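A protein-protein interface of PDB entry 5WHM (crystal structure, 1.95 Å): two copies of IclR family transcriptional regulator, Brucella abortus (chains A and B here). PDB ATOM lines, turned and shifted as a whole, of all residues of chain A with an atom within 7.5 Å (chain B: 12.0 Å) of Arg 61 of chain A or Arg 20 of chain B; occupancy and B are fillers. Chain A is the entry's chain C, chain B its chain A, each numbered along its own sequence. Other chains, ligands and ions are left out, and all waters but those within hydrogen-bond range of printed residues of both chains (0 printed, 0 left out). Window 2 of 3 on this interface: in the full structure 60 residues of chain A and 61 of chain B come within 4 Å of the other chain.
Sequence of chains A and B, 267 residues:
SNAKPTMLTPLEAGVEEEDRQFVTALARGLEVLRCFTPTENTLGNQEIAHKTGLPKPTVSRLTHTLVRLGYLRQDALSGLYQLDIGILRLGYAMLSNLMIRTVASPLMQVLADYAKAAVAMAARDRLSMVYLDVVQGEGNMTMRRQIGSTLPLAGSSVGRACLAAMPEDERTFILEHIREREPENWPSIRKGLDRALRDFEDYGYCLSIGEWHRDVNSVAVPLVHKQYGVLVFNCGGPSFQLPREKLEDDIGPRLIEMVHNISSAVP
The side-chain carboxylate (OD2) of Asp 19 of chain B sits at hydrogen-bond distance from a ring nitrogen (NE2) of His 64 of chain A (2.8 Å).
The backbone NH of Met 7 of chain B is in hydrogen-bond range of the backbone carbonyl oxygen of Arg 68 of chain A (3.0 Å).
The backbone carbonyl oxygen (O) of Gln 21 of chain B lies within hydrogen-bond range of the guanidinium group (NE) of Arg 61 of chain A, 3.2 Å away.
The backbone NH (N) of Val 23 of chain B is in hydrogen-bond range of the side-chain hydroxyl (OG1) of Thr 65 of chain A (2.9 Å).
OE2 of Glu 16 of chain B is in salt-bridge range of NH2 of Arg 68 of chain A (3.0 Å).
OD2 of Asp 19 of chain B lies within salt-bridge range of NH1 of Arg 68 of chain A.
The side-chain carboxylate (OD1) of Asp 19 of chain B lies within hydrogen-bond range of the backbone NH (N) of Gln 21 of chain B.
NH2 of Arg 20 of chain B is in salt-bridge range of OE1 of Glu 18 of chain B, at 2.5 Å.
The backbone carbonyl oxygen (O) of Arg 61 of chain A lies within hydrogen-bond range of the side-chain hydroxyl (OG1) of Thr 65 of chain A.
The backbone NH (N) of Phe 22 of chain B is in hydrogen-bond range of the side-chain carboxylate (OD1) of Asp 19 of chain B, 3.3 Å away.
Among the printed residues, pairs that only touch across the chains: Arg 61 of chain A with Arg 20 of chain B (3.6 Å), Arg 61 of chain A with Phe 22 of chain B (3.6 Å), Arg 61 of chain A with Val 23 of chain B (3.9 Å), Leu 62 of chain A with Leu 26 of chain B (3.9 Å), His 64 of chain A with Gln 21 of chain B (3.6 Å), Thr 65 of chain A with Gln 21 of chain B (3.6 Å), Thr 65 of chain A with Phe 22 of chain B (3.5 Å), Leu 66 of chain A with Leu 26 of chain B (3.8 Å) and Leu 66 of chain A with Leu 30 of chain B (3.7 Å).
Printed residues of chain B within 4 Å of Arg 61 of chain A: Arg 20 (3.6 Å), Gln 21 (3.2 Å), Phe 22 (3.6 Å) and Val 23 (3.9 Å).
Printed residues of chain A within 4 Å of Arg 20 of chain B: Arg 61 (3.6 Å).
Pro 57 of chain A touches none of the printed residues of chain B.
Leu 62 of chain A touches one residue of chain B.
No residue of chain B comes within 4 Å of Thr 63 of chain A.
Of the printed residues of chain A, Met 7 of chain B touches Arg 68 (3.0 Å).
Printed residues of chain B within 4 Å of Thr 65 of chain A: Gln 21 (3.6 Å), Phe 22 (3.5 Å) and Val 23 (2.9 Å).
Of the printed residues of chain A, Phe 22 of chain B touches Arg 61 and Thr 65.
The nearest printed residue of chain A that does not touch Val 23 of chain B is Leu 62 of chain A (4.1 Å).
Of the 15 printed residues of chain B, 9 touch a printed residue of chain A.
Printed residues of chain B that touch a printed residue of chain A: Met 7, Glu 16, Asp 19, Arg 20, Gln 21, Phe 22, Val 23, Leu 26 and Leu 30.
Among the printed residues, 15 pairs touch across the chains.
Among the printed residues, Asp or Glu carboxylates within 4 Å of a Lys or Arg side-chain nitrogen of the other chain: Arg 68 of chain A with Glu 16 of chain B and Arg 68 of chain A with Asp 19 of chain B.
No position is printed for both chains.
Of the 15 pairs that touch across the chains among the printed residues, none has its exchanged pair printed and touching as well.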
ATOM      1  N   ASN A  45       9.333 -14.300 -32.802  1.00  0.00           N
ATOM      2  CA  ASN A  45       9.306 -13.131 -31.924  1.00  0.00           C
ATOM      3  C   ASN A  45       9.830 -11.878 -32.638  1.00  0.00           C
ATOM      4  O   ASN A  45       9.276 -10.790 -32.466  1.00  0.00           O
ATOM      5  CB  ASN A  45      10.106 -13.415 -30.630  1.00  0.00           C
ATOM      6  CG  ASN A  45       9.329 -14.333 -29.614  1.00  0.00           C
ATOM      7  OD1 ASN A  45       8.142 -14.139 -29.356  1.00  0.00           O
ATOM      8  ND2 ASN A  45      10.019 -15.318 -29.046  1.00  0.00           N
ATOM      9  N   PRO A  55       9.218  -3.990 -27.906  1.00  0.00           N
ATOM     10  CA  PRO A  55      10.523  -4.641 -27.695  1.00  0.00           C
ATOM     11  C   PRO A  55      10.413  -6.168 -27.706  1.00  0.00           C
ATOM     12  O   PRO A  55       9.410  -6.759 -27.288  1.00  0.00           O
ATOM     13  CB  PRO A  55      10.963  -4.121 -26.316  1.00  0.00           C
ATOM     14  CG  PRO A  55      10.141  -2.884 -26.078  1.00  0.00           C
ATOM     15  CD  PRO A  55       8.818  -3.157 -26.758  1.00  0.00           C
ATOM     16  N   LYS A  56      11.477  -6.809 -28.180  1.00  0.00           N
ATOM     17  CA  LYS A  56      11.511  -8.269 -28.225  1.00  0.00           C
ATOM     18  C   LYS A  56      11.271  -8.965 -26.878  1.00  0.00           C
ATOM     19  O   LYS A  56      10.535  -9.968 -26.868  1.00  0.00           O
ATOM     20  CB  LYS A  56      12.838  -8.728 -28.851  1.00  0.00           C
ATOM     21  CG  LYS A  56      12.744 -10.103 -29.528  1.00  0.00           C
ATOM     22  CD  LYS A  56      14.125 -10.658 -29.904  1.00  0.00           C
ATOM     23  CE  LYS A  56      14.065 -12.143 -30.269  1.00  0.00           C
ATOM     24  NZ  LYS A  56      15.316 -12.888 -29.867  1.00  0.00           N
ATOM     25  N   PRO A  57      11.836  -8.533 -25.732  1.00  0.00           N
ATOM     26  CA  PRO A  57      11.479  -9.213 -24.465  1.00  0.00           C
ATOM     27  C   PRO A  57       9.999  -9.089 -24.140  1.00  0.00           C
ATOM     28  O   PRO A  57       9.418  -9.999 -23.541  1.00  0.00           O
ATOM     29  CB  PRO A  57      12.349  -8.509 -23.404  1.00  0.00           C
ATOM     30  CG  PRO A  57      13.409  -7.774 -24.171  1.00  0.00           C
ATOM     31  CD  PRO A  57      12.797  -7.432 -25.510  1.00  0.00           C
ATOM     32  N   THR A  58       9.362  -7.987 -24.543  1.00  0.00           N
ATOM     33  CA  THR A  58       7.934  -7.828 -24.295  1.00  0.00           C
ATOM     34  C   THR A  58       7.128  -8.803 -25.136  1.00  0.00           C
ATOM     35  O   THR A  58       6.228  -9.488 -24.633  1.00  0.00           O
ATOM     36  CB  THR A  58       7.531  -6.390 -24.599  1.00  0.00           C
ATOM     37  OG1 THR A  58       8.187  -5.541 -23.671  1.00  0.00           O
ATOM     38  CG2 THR A  58       6.015  -6.194 -24.483  1.00  0.00           C
ATOM     39  N   VAL A  59       7.442  -8.875 -26.431  1.00  0.00           N
ATOM     40  CA  VAL A  59       6.798  -9.843 -27.304  1.00  0.00           C
ATOM     41  C   VAL A  59       7.001 -11.261 -26.761  1.00  0.00           C
ATOM     42  O   VAL A  59       6.060 -12.063 -26.748  1.00  0.00           O
ATOM     43  CB  VAL A  59       7.348  -9.697 -28.733  1.00  0.00           C
ATOM     44  CG1 VAL A  59       6.869 -10.858 -29.619  1.00  0.00           C
ATOM     45  CG2 VAL A  59       6.951  -8.322 -29.294  1.00  0.00           C
ATOM     46  N   SER A  60       8.223 -11.555 -26.288  1.00  0.00           N
ATOM     47  CA  SER A  60       8.533 -12.892 -25.767  1.00  0.00           C
ATOM     48  C   SER A  60       7.612 -13.287 -24.623  1.00  0.00           C
ATOM     49  O   SER A  60       7.176 -14.442 -24.550  1.00  0.00           O
ATOM     50  CB  SER A  60       9.989 -12.960 -25.301  1.00  0.00           C
ATOM     51  OG  SER A  60      10.867 -13.018 -26.403  1.00  0.00           O
ATOM     52  N   ARG A  61       7.333 -12.365 -23.695  1.00  0.00           N
ATOM     53  CA  ARG A  61       6.396 -12.682 -22.614  1.00  0.00           C
ATOM     54  C   ARG A  61       4.995 -12.925 -23.161  1.00  0.00           C
ATOM     55  O   ARG A  61       4.300 -13.850 -22.724  1.00  0.00           O
ATOM     56  CB  ARG A  61       6.357 -11.552 -21.574  1.00  0.00           C
ATOM     57  CG  ARG A  61       7.661 -11.287 -20.821  1.00  0.00           C
ATOM     58  CD  ARG A  61       7.447 -10.217 -19.741  1.00  0.00           C
ATOM     59  NE  ARG A  61       6.443 -10.664 -18.779  1.00  0.00           N
ATOM     60  CZ  ARG A  61       5.919  -9.910 -17.823  1.00  0.00           C
ATOM     61  NH1 ARG A  61       6.311  -8.651 -17.675  1.00  0.00           N
ATOM     62  NH2 ARG A  61       5.009 -10.424 -17.008  1.00  0.00           N
ATOM     63  N   LEU A  62       4.560 -12.100 -24.124  1.00  0.00           N
ATOM     64  CA  LEU A  62       3.206 -12.234 -24.661  1.00  0.00           C
ATOM     65  C   LEU A  62       3.018 -13.561 -25.394  1.00  0.00           C
ATOM     66  O   LEU A  62       2.018 -14.268 -25.165  1.00  0.00           O
ATOM     67  CB  LEU A  62       2.889 -11.046 -25.583  1.00  0.00           C
ATOM     68  CG  LEU A  62       2.932  -9.697 -24.861  1.00  0.00           C
ATOM     69  CD1 LEU A  62       2.980  -8.523 -25.869  1.00  0.00           C
ATOM     70  CD2 LEU A  62       1.732  -9.611 -23.932  1.00  0.00           C
ATOM     71  N   THR A  63       3.973 -13.927 -26.261  1.00  0.00           N
ATOM     72  CA  THR A  63       3.837 -15.185 -26.985  1.00  0.00           C
ATOM     73  C   THR A  63       3.961 -16.380 -26.048  1.00  0.00           C
ATOM     74  O   THR A  63       3.237 -17.365 -26.217  1.00  0.00           O
ATOM     75  CB  THR A  63       4.846 -15.298 -28.141  1.00  0.00           C
ATOM     76  OG1 THR A  63       6.169 -15.140 -27.655  1.00  0.00           O
ATOM     77  CG2 THR A  63       4.598 -14.227 -29.270  1.00  0.00           C
ATOM     78  N   HIS A  64       4.873 -16.322 -25.067  1.00  0.00           N
ATOM     79  CA  HIS A  64       4.956 -17.398 -24.071  1.00  0.00           C
ATOM     80  C   HIS A  64       3.614 -17.602 -23.383  1.00  0.00           C
ATOM     81  O   HIS A  64       3.137 -18.738 -23.235  1.00  0.00           O
ATOM     82  CB  HIS A  64       6.036 -17.077 -23.033  1.00  0.00           C
ATOM     83  CG  HIS A  64       5.965 -17.943 -21.810  1.00  0.00           C
ATOM     84  ND1 HIS A  64       6.504 -19.209 -21.773  1.00  0.00           N
ATOM     85  CD2 HIS A  64       5.417 -17.727 -20.588  1.00  0.00           C
ATOM     86  CE1 HIS A  64       6.305 -19.735 -20.571  1.00  0.00           C
ATOM     87  NE2 HIS A  64       5.662 -18.850 -19.826  1.00  0.00           N
ATOM     88  N   THR A  65       2.993 -16.497 -22.950  1.00  0.00           N
ATOM     89  CA  THR A  65       1.674 -16.568 -22.325  1.00  0.00           C
ATOM     90  C   THR A  65       0.632 -17.179 -23.271  1.00  0.00           C
ATOM     91  O   THR A  65      -0.174 -18.031 -22.869  1.00  0.00           O
ATOM     92  CB  THR A  65       1.278 -15.150 -21.896  1.00  0.00           C
ATOM     93  OG1 THR A  65       2.285 -14.677 -21.012  1.00  0.00           O
ATOM     94  CG2 THR A  65      -0.102 -15.104 -21.204  1.00  0.00           C
ATOM     95  N   LEU A  66       0.602 -16.718 -24.524  1.00  0.00           N
ATOM     96  CA  LEU A  66      -0.405 -17.198 -25.467  1.00  0.00           C
ATOM     97  C   LEU A  66      -0.222 -18.690 -25.747  1.00  0.00           C
ATOM     98  O   LEU A  66      -1.205 -19.423 -25.899  1.00  0.00           O
ATOM     99  CB  LEU A  66      -0.342 -16.359 -26.768  1.00  0.00           C
ATOM    100  CG  LEU A  66      -0.798 -14.910 -26.561  1.00  0.00           C
ATOM    101  CD1 LEU A  66      -0.395 -13.994 -27.778  1.00  0.00           C
ATOM    102  CD2 LEU A  66      -2.314 -14.863 -26.336  1.00  0.00           C
ATOM    103  N   VAL A  67       1.031 -19.163 -25.798  1.00  0.00           N
ATOM    104  CA  VAL A  67       1.274 -20.601 -25.960  1.00  0.00           C
ATOM    105  C   VAL A  67       0.781 -21.389 -24.743  1.00  0.00           C
ATOM    106  O   VAL A  67       0.103 -22.414 -24.881  1.00  0.00           O
ATOM    107  CB  VAL A  67       2.763 -20.860 -26.249  1.00  0.00           C
ATOM    108  CG1 VAL A  67       3.071 -22.391 -26.245  1.00  0.00           C
ATOM    109  CG2 VAL A  67       3.140 -20.197 -27.596  1.00  0.00           C
ATOM    110  N   ARG A  68       1.100 -20.929 -23.533  1.00  0.00           N
ATOM    111  CA  ARG A  68       0.649 -21.701 -22.373  1.00  0.00           C
ATOM    112  C   ARG A  68      -0.872 -21.770 -22.313  1.00  0.00           C
ATOM    113  O   ARG A  68      -1.431 -22.748 -21.807  1.00  0.00           O
ATOM    114  CB  ARG A  68       1.203 -21.117 -21.075  1.00  0.00           C
ATOM    115  CG  ARG A  68       2.684 -21.355 -20.900  1.00  0.00           C
ATOM    116  CD  ARG A  68       3.107 -21.242 -19.441  1.00  0.00           C
ATOM    117  NE  ARG A  68       2.458 -22.242 -18.597  1.00  0.00           N
ATOM    118  CZ  ARG A  68       2.453 -22.197 -17.270  1.00  0.00           C
ATOM    119  NH1 ARG A  68       3.056 -21.181 -16.653  1.00  0.00           N
ATOM    120  NH2 ARG A  68       1.836 -23.153 -16.566  1.00  0.00           N
ATOM    121  N   TYR A  81       5.764 -19.504 -34.210  1.00  0.00           N
ATOM    122  CA  TYR A  81       4.404 -19.590 -33.694  1.00  0.00           C
ATOM    123  C   TYR A  81       3.363 -19.615 -34.815  1.00  0.00           C
ATOM    124  O   TYR A  81       3.563 -19.052 -35.900  1.00  0.00           O
ATOM    125  CB  TYR A  81       4.057 -18.410 -32.781  1.00  0.00           C
ATOM    126  CG  TYR A  81       5.083 -18.215 -31.682  1.00  0.00           C
ATOM    127  CD1 TYR A  81       5.036 -18.976 -30.501  1.00  0.00           C
ATOM    128  CD2 TYR A  81       6.115 -17.314 -31.844  1.00  0.00           C
ATOM    129  CE1 TYR A  81       6.012 -18.794 -29.478  1.00  0.00           C
ATOM    130  CE2 TYR A  81       7.086 -17.135 -30.855  1.00  0.00           C
ATOM    131  CZ  TYR A  81       7.026 -17.876 -29.685  1.00  0.00           C
ATOM    132  OH  TYR A  81       8.012 -17.684 -28.736  1.00  0.00           O
ATOM    133  N   MET B   7      -2.600 -25.078 -20.237  1.00  0.00           N
ATOM    134  CA  MET B   7      -3.344 -24.788 -19.016  1.00  0.00           C
ATOM    135  C   MET B   7      -4.836 -25.040 -19.160  1.00  0.00           C
ATOM    136  O   MET B   7      -5.497 -24.529 -20.085  1.00  0.00           O
ATOM    137  CB  MET B   7      -3.128 -23.338 -18.604  1.00  0.00           C
ATOM    138  CG  MET B   7      -1.728 -23.023 -18.152  1.00  0.00           C
ATOM    139  SD  MET B   7      -1.550 -21.093 -17.928  1.00  0.00           S
ATOM    140  CE  MET B   7      -1.358 -21.027 -15.980  1.00  0.00           C
ATOM    141  N   GLU B  16       1.393 -25.416  -9.662  1.00  0.00           N
ATOM    142  CA  GLU B  16       2.298 -24.794 -10.627  1.00  0.00           C
ATOM    143  C   GLU B  16       3.283 -23.851  -9.950  1.00  0.00           C
ATOM    144  O   GLU B  16       2.879 -22.909  -9.260  1.00  0.00           O
ATOM    145  CB  GLU B  16       1.484 -24.020 -11.664  1.00  0.00           C
ATOM    146  CG  GLU B  16       0.628 -24.862 -12.588  1.00  0.00           C
ATOM    147  CD  GLU B  16      -0.445 -24.036 -13.272  1.00  0.00           C
ATOM    148  OE1 GLU B  16      -1.553 -23.927 -12.704  1.00  0.00           O
ATOM    149  OE2 GLU B  16      -0.175 -23.477 -14.361  1.00  0.00           O
ATOM    150  N   GLU B  17       4.577 -24.095 -10.152  1.00  0.00           N
ATOM    151  CA  GLU B  17       5.565 -23.139  -9.680  1.00  0.00           C
ATOM    152  C   GLU B  17       5.440 -21.836 -10.467  1.00  0.00           C
ATOM    153  O   GLU B  17       4.925 -21.799 -11.587  1.00  0.00           O
ATOM    154  CB  GLU B  17       6.983 -23.706  -9.786  1.00  0.00           C
ATOM    155  CG  GLU B  17       7.401 -24.507  -8.569  1.00  0.00           C
ATOM    156  CD  GLU B  17       8.902 -24.734  -8.492  1.00  0.00           C
ATOM    157  OE1 GLU B  17       9.631 -24.167  -9.341  1.00  0.00           O
ATOM    158  OE2 GLU B  17       9.347 -25.479  -7.583  1.00  0.00           O
ATOM    159  N   GLU B  18       5.896 -20.752  -9.852  1.00  0.00           N
ATOM    160  CA  GLU B  18       5.565 -19.439 -10.353  1.00  0.00           C
ATOM    161  C   GLU B  18       6.202 -19.231 -11.726  1.00  0.00           C
ATOM    162  O   GLU B  18       7.204 -19.851 -12.092  1.00  0.00           O
ATOM    163  CB  GLU B  18       5.993 -18.351  -9.362  1.00  0.00           C
ATOM    164  CG  GLU B  18       7.457 -18.288  -9.060  1.00  0.00           C
ATOM    165  CD  GLU B  18       7.794 -17.342  -7.891  1.00  0.00           C
ATOM    166  OE1 GLU B  18       8.491 -16.330  -8.118  1.00  0.00           O
ATOM    167  OE2 GLU B  18       7.373 -17.610  -6.742  1.00  0.00           O
ATOM    168  N   ASP B  19       5.563 -18.402 -12.509  1.00  0.00           N
ATOM    169  CA  ASP B  19       6.010 -18.141 -13.865  1.00  0.00           C
ATOM    170  C   ASP B  19       6.070 -16.629 -13.989  1.00  0.00           C
ATOM    171  O   ASP B  19       5.029 -15.978 -14.093  1.00  0.00           O
ATOM    172  CB  ASP B  19       5.051 -18.775 -14.873  1.00  0.00           C
ATOM    173  CG  ASP B  19       5.455 -18.527 -16.322  1.00  0.00           C
ATOM    174  OD1 ASP B  19       6.360 -17.696 -16.585  1.00  0.00           O
ATOM    175  OD2 ASP B  19       4.855 -19.196 -17.198  1.00  0.00           O
ATOM    176  N   ARG B  20       7.278 -16.076 -13.954  1.00  0.00           N
ATOM    177  CA  ARG B  20       7.414 -14.630 -13.998  1.00  0.00           C
ATOM    178  C   ARG B  20       7.275 -14.064 -15.407  1.00  0.00           C
ATOM    179  O   ARG B  20       7.177 -12.842 -15.551  1.00  0.00           O
ATOM    180  CB  ARG B  20       8.750 -14.206 -13.353  1.00  0.00           C
ATOM    181  CG  ARG B  20       8.831 -14.660 -11.895  1.00  0.00           C
ATOM    182  CD  ARG B  20       9.354 -13.616 -10.917  1.00  0.00           C
ATOM    183  NE  ARG B  20       9.204 -14.158  -9.567  1.00  0.00           N
ATOM    184  CZ  ARG B  20       9.219 -13.450  -8.446  1.00  0.00           C
ATOM    185  NH1 ARG B  20       9.385 -12.140  -8.489  1.00  0.00           N
ATOM    186  NH2 ARG B  20       9.067 -14.071  -7.283  1.00  0.00           N
ATOM    187  N   GLN B  21       7.252 -14.923 -16.438  1.00  0.00           N
ATOM    188  CA  GLN B  21       6.986 -14.492 -17.808  1.00  0.00           C
ATOM    189  C   GLN B  21       5.494 -14.346 -18.094  1.00  0.00           C
ATOM    190  O   GLN B  21       5.118 -13.617 -19.020  1.00  0.00           O
ATOM    191  CB  GLN B  21       7.558 -15.494 -18.826  1.00  0.00           C
ATOM    192  CG  GLN B  21       9.029 -15.854 -18.704  1.00  0.00           C
ATOM    193  CD  GLN B  21       9.854 -14.763 -18.070  1.00  0.00           C
ATOM    194  OE1 GLN B  21      10.436 -14.951 -16.996  1.00  0.00           O
ATOM    195  NE2 GLN B  21       9.913 -13.606 -18.726  1.00  0.00           N
ATOM    196  N   PHE B  22       4.646 -15.018 -17.326  1.00  0.00           N
ATOM    197  CA  PHE B  22       3.230 -15.117 -17.659  1.00  0.00           C
ATOM    198  C   PHE B  22       2.545 -13.757 -17.513  1.00  0.00           C
ATOM    199  O   PHE B  22       2.694 -13.091 -16.482  1.00  0.00           O
ATOM    200  CB  PHE B  22       2.576 -16.149 -16.755  1.00  0.00           C
ATOM    201  CG  PHE B  22       1.169 -16.508 -17.142  1.00  0.00           C
ATOM    202  CD1 PHE B  22       0.932 -17.397 -18.185  1.00  0.00           C
ATOM    203  CD2 PHE B  22       0.089 -16.009 -16.437  1.00  0.00           C
ATOM    204  CE1 PHE B  22      -0.384 -17.773 -18.537  1.00  0.00           C
ATOM    205  CE2 PHE B  22      -1.234 -16.377 -16.791  1.00  0.00           C
ATOM    206  CZ  PHE B  22      -1.454 -17.262 -17.835  1.00  0.00           C
ATOM    207  N   VAL B  23       1.766 -13.362 -18.522  1.00  0.00           N
ATOM    208  CA  VAL B  23       1.130 -12.041 -18.538  1.00  0.00           C
ATOM    209  C   VAL B  23      -0.326 -12.212 -18.130  1.00  0.00           C
ATOM    210  O   VAL B  23      -1.201 -12.479 -18.961  1.00  0.00           O
ATOM    211  CB  VAL B  23       1.259 -11.347 -19.898  1.00  0.00           C
ATOM    212  CG1 VAL B  23       0.555  -9.995 -19.845  1.00  0.00           C
ATOM    213  CG2 VAL B  23       2.761 -11.150 -20.253  1.00  0.00           C
ATOM    214  N   THR B  24      -0.581 -11.983 -16.845  1.00  0.00           N
ATOM    215  CA  THR B  24      -1.874 -12.284 -16.237  1.00  0.00           C
ATOM    216  C   THR B  24      -3.018 -11.499 -16.878  1.00  0.00           C
ATOM    217  O   THR B  24      -4.109 -12.050 -17.080  1.00  0.00           O
ATOM    218  CB  THR B  24      -1.783 -11.995 -14.727  1.00  0.00           C
ATOM    219  OG1 THR B  24      -0.786 -12.857 -14.175  1.00  0.00           O
ATOM    220  CG2 THR B  24      -3.096 -12.277 -14.044  1.00  0.00           C
ATOM    221  N   ALA B  25      -2.799 -10.213 -17.213  1.00  0.00           N
ATOM    222  CA  ALA B  25      -3.881  -9.399 -17.769  1.00  0.00           C
ATOM    223  C   ALA B  25      -4.330  -9.913 -19.130  1.00  0.00           C
ATOM    224  O   ALA B  25      -5.510  -9.785 -19.490  1.00  0.00           O
ATOM    225  CB  ALA B  25      -3.447  -7.932 -17.908  1.00  0.00           C
ATOM    226  N   LEU B  26      -3.397 -10.455 -19.910  1.00  0.00           N
ATOM    227  CA  LEU B  26      -3.745 -11.027 -21.204  1.00  0.00           C
ATOM    228  C   LEU B  26      -4.602 -12.267 -21.006  1.00  0.00           C
ATOM    229  O   LEU B  26      -5.642 -12.428 -21.662  1.00  0.00           O
ATOM    230  CB  LEU B  26      -2.470 -11.362 -21.991  1.00  0.00           C
ATOM    231  CG  LEU B  26      -2.598 -12.053 -23.351  1.00  0.00           C
ATOM    232  CD1 LEU B  26      -3.575 -11.203 -24.271  1.00  0.00           C
ATOM    233  CD2 LEU B  26      -1.170 -12.171 -23.928  1.00  0.00           C
ATOM    234  N   ALA B  27      -4.187 -13.139 -20.086  1.00  0.00           N
ATOM    235  CA  ALA B  27      -4.960 -14.344 -19.783  1.00  0.00           C
ATOM    236  C   ALA B  27      -6.382 -13.978 -19.393  1.00  0.00           C
ATOM    237  O   ALA B  27      -7.343 -14.518 -19.940  1.00  0.00           O
ATOM    238  CB  ALA B  27      -4.300 -15.134 -18.654  1.00  0.00           C
ATOM    239  N   ARG B  28      -6.529 -13.004 -18.488  1.00  0.00           N
ATOM    240  CA  ARG B  28      -7.845 -12.652 -17.976  1.00  0.00           C
ATOM    241  C   ARG B  28      -8.742 -12.079 -19.064  1.00  0.00           C
ATOM    242  O   ARG B  28      -9.932 -12.398 -19.121  1.00  0.00           O
ATOM    243  CB  ARG B  28      -7.704 -11.638 -16.844  1.00  0.00           C
ATOM    244  CG  ARG B  28      -7.149 -12.235 -15.555  1.00  0.00           C
ATOM    245  CD  ARG B  28      -6.911 -11.126 -14.539  1.00  0.00           C
ATOM    246  NE  ARG B  28      -6.449 -11.710 -13.278  1.00  0.00           N
ATOM    247  CZ  ARG B  28      -6.069 -10.988 -12.230  1.00  0.00           C
ATOM    248  NH1 ARG B  28      -5.673 -11.590 -11.118  1.00  0.00           N
ATOM    249  NH2 ARG B  28      -6.061  -9.667 -12.318  1.00  0.00           N
ATOM    250  N   LEU B  30      -8.666 -12.502 -22.331  1.00  0.00           N
ATOM    251  CA  LEU B  30      -9.153 -13.556 -23.236  1.00  0.00           C
ATOM    252  C   LEU B  30     -10.177 -14.468 -22.546  1.00  0.00           C
ATOM    253  O   LEU B  30     -11.140 -14.913 -23.188  1.00  0.00           O
ATOM    254  CB  LEU B  30      -7.969 -14.352 -23.796  1.00  0.00           C
ATOM    255  CG  LEU B  30      -7.058 -13.458 -24.664  1.00  0.00           C
ATOM    256  CD1 LEU B  30      -5.752 -14.150 -25.091  1.00  0.00           C
ATOM    257  CD2 LEU B  30      -7.809 -12.906 -25.889  1.00  0.00           C
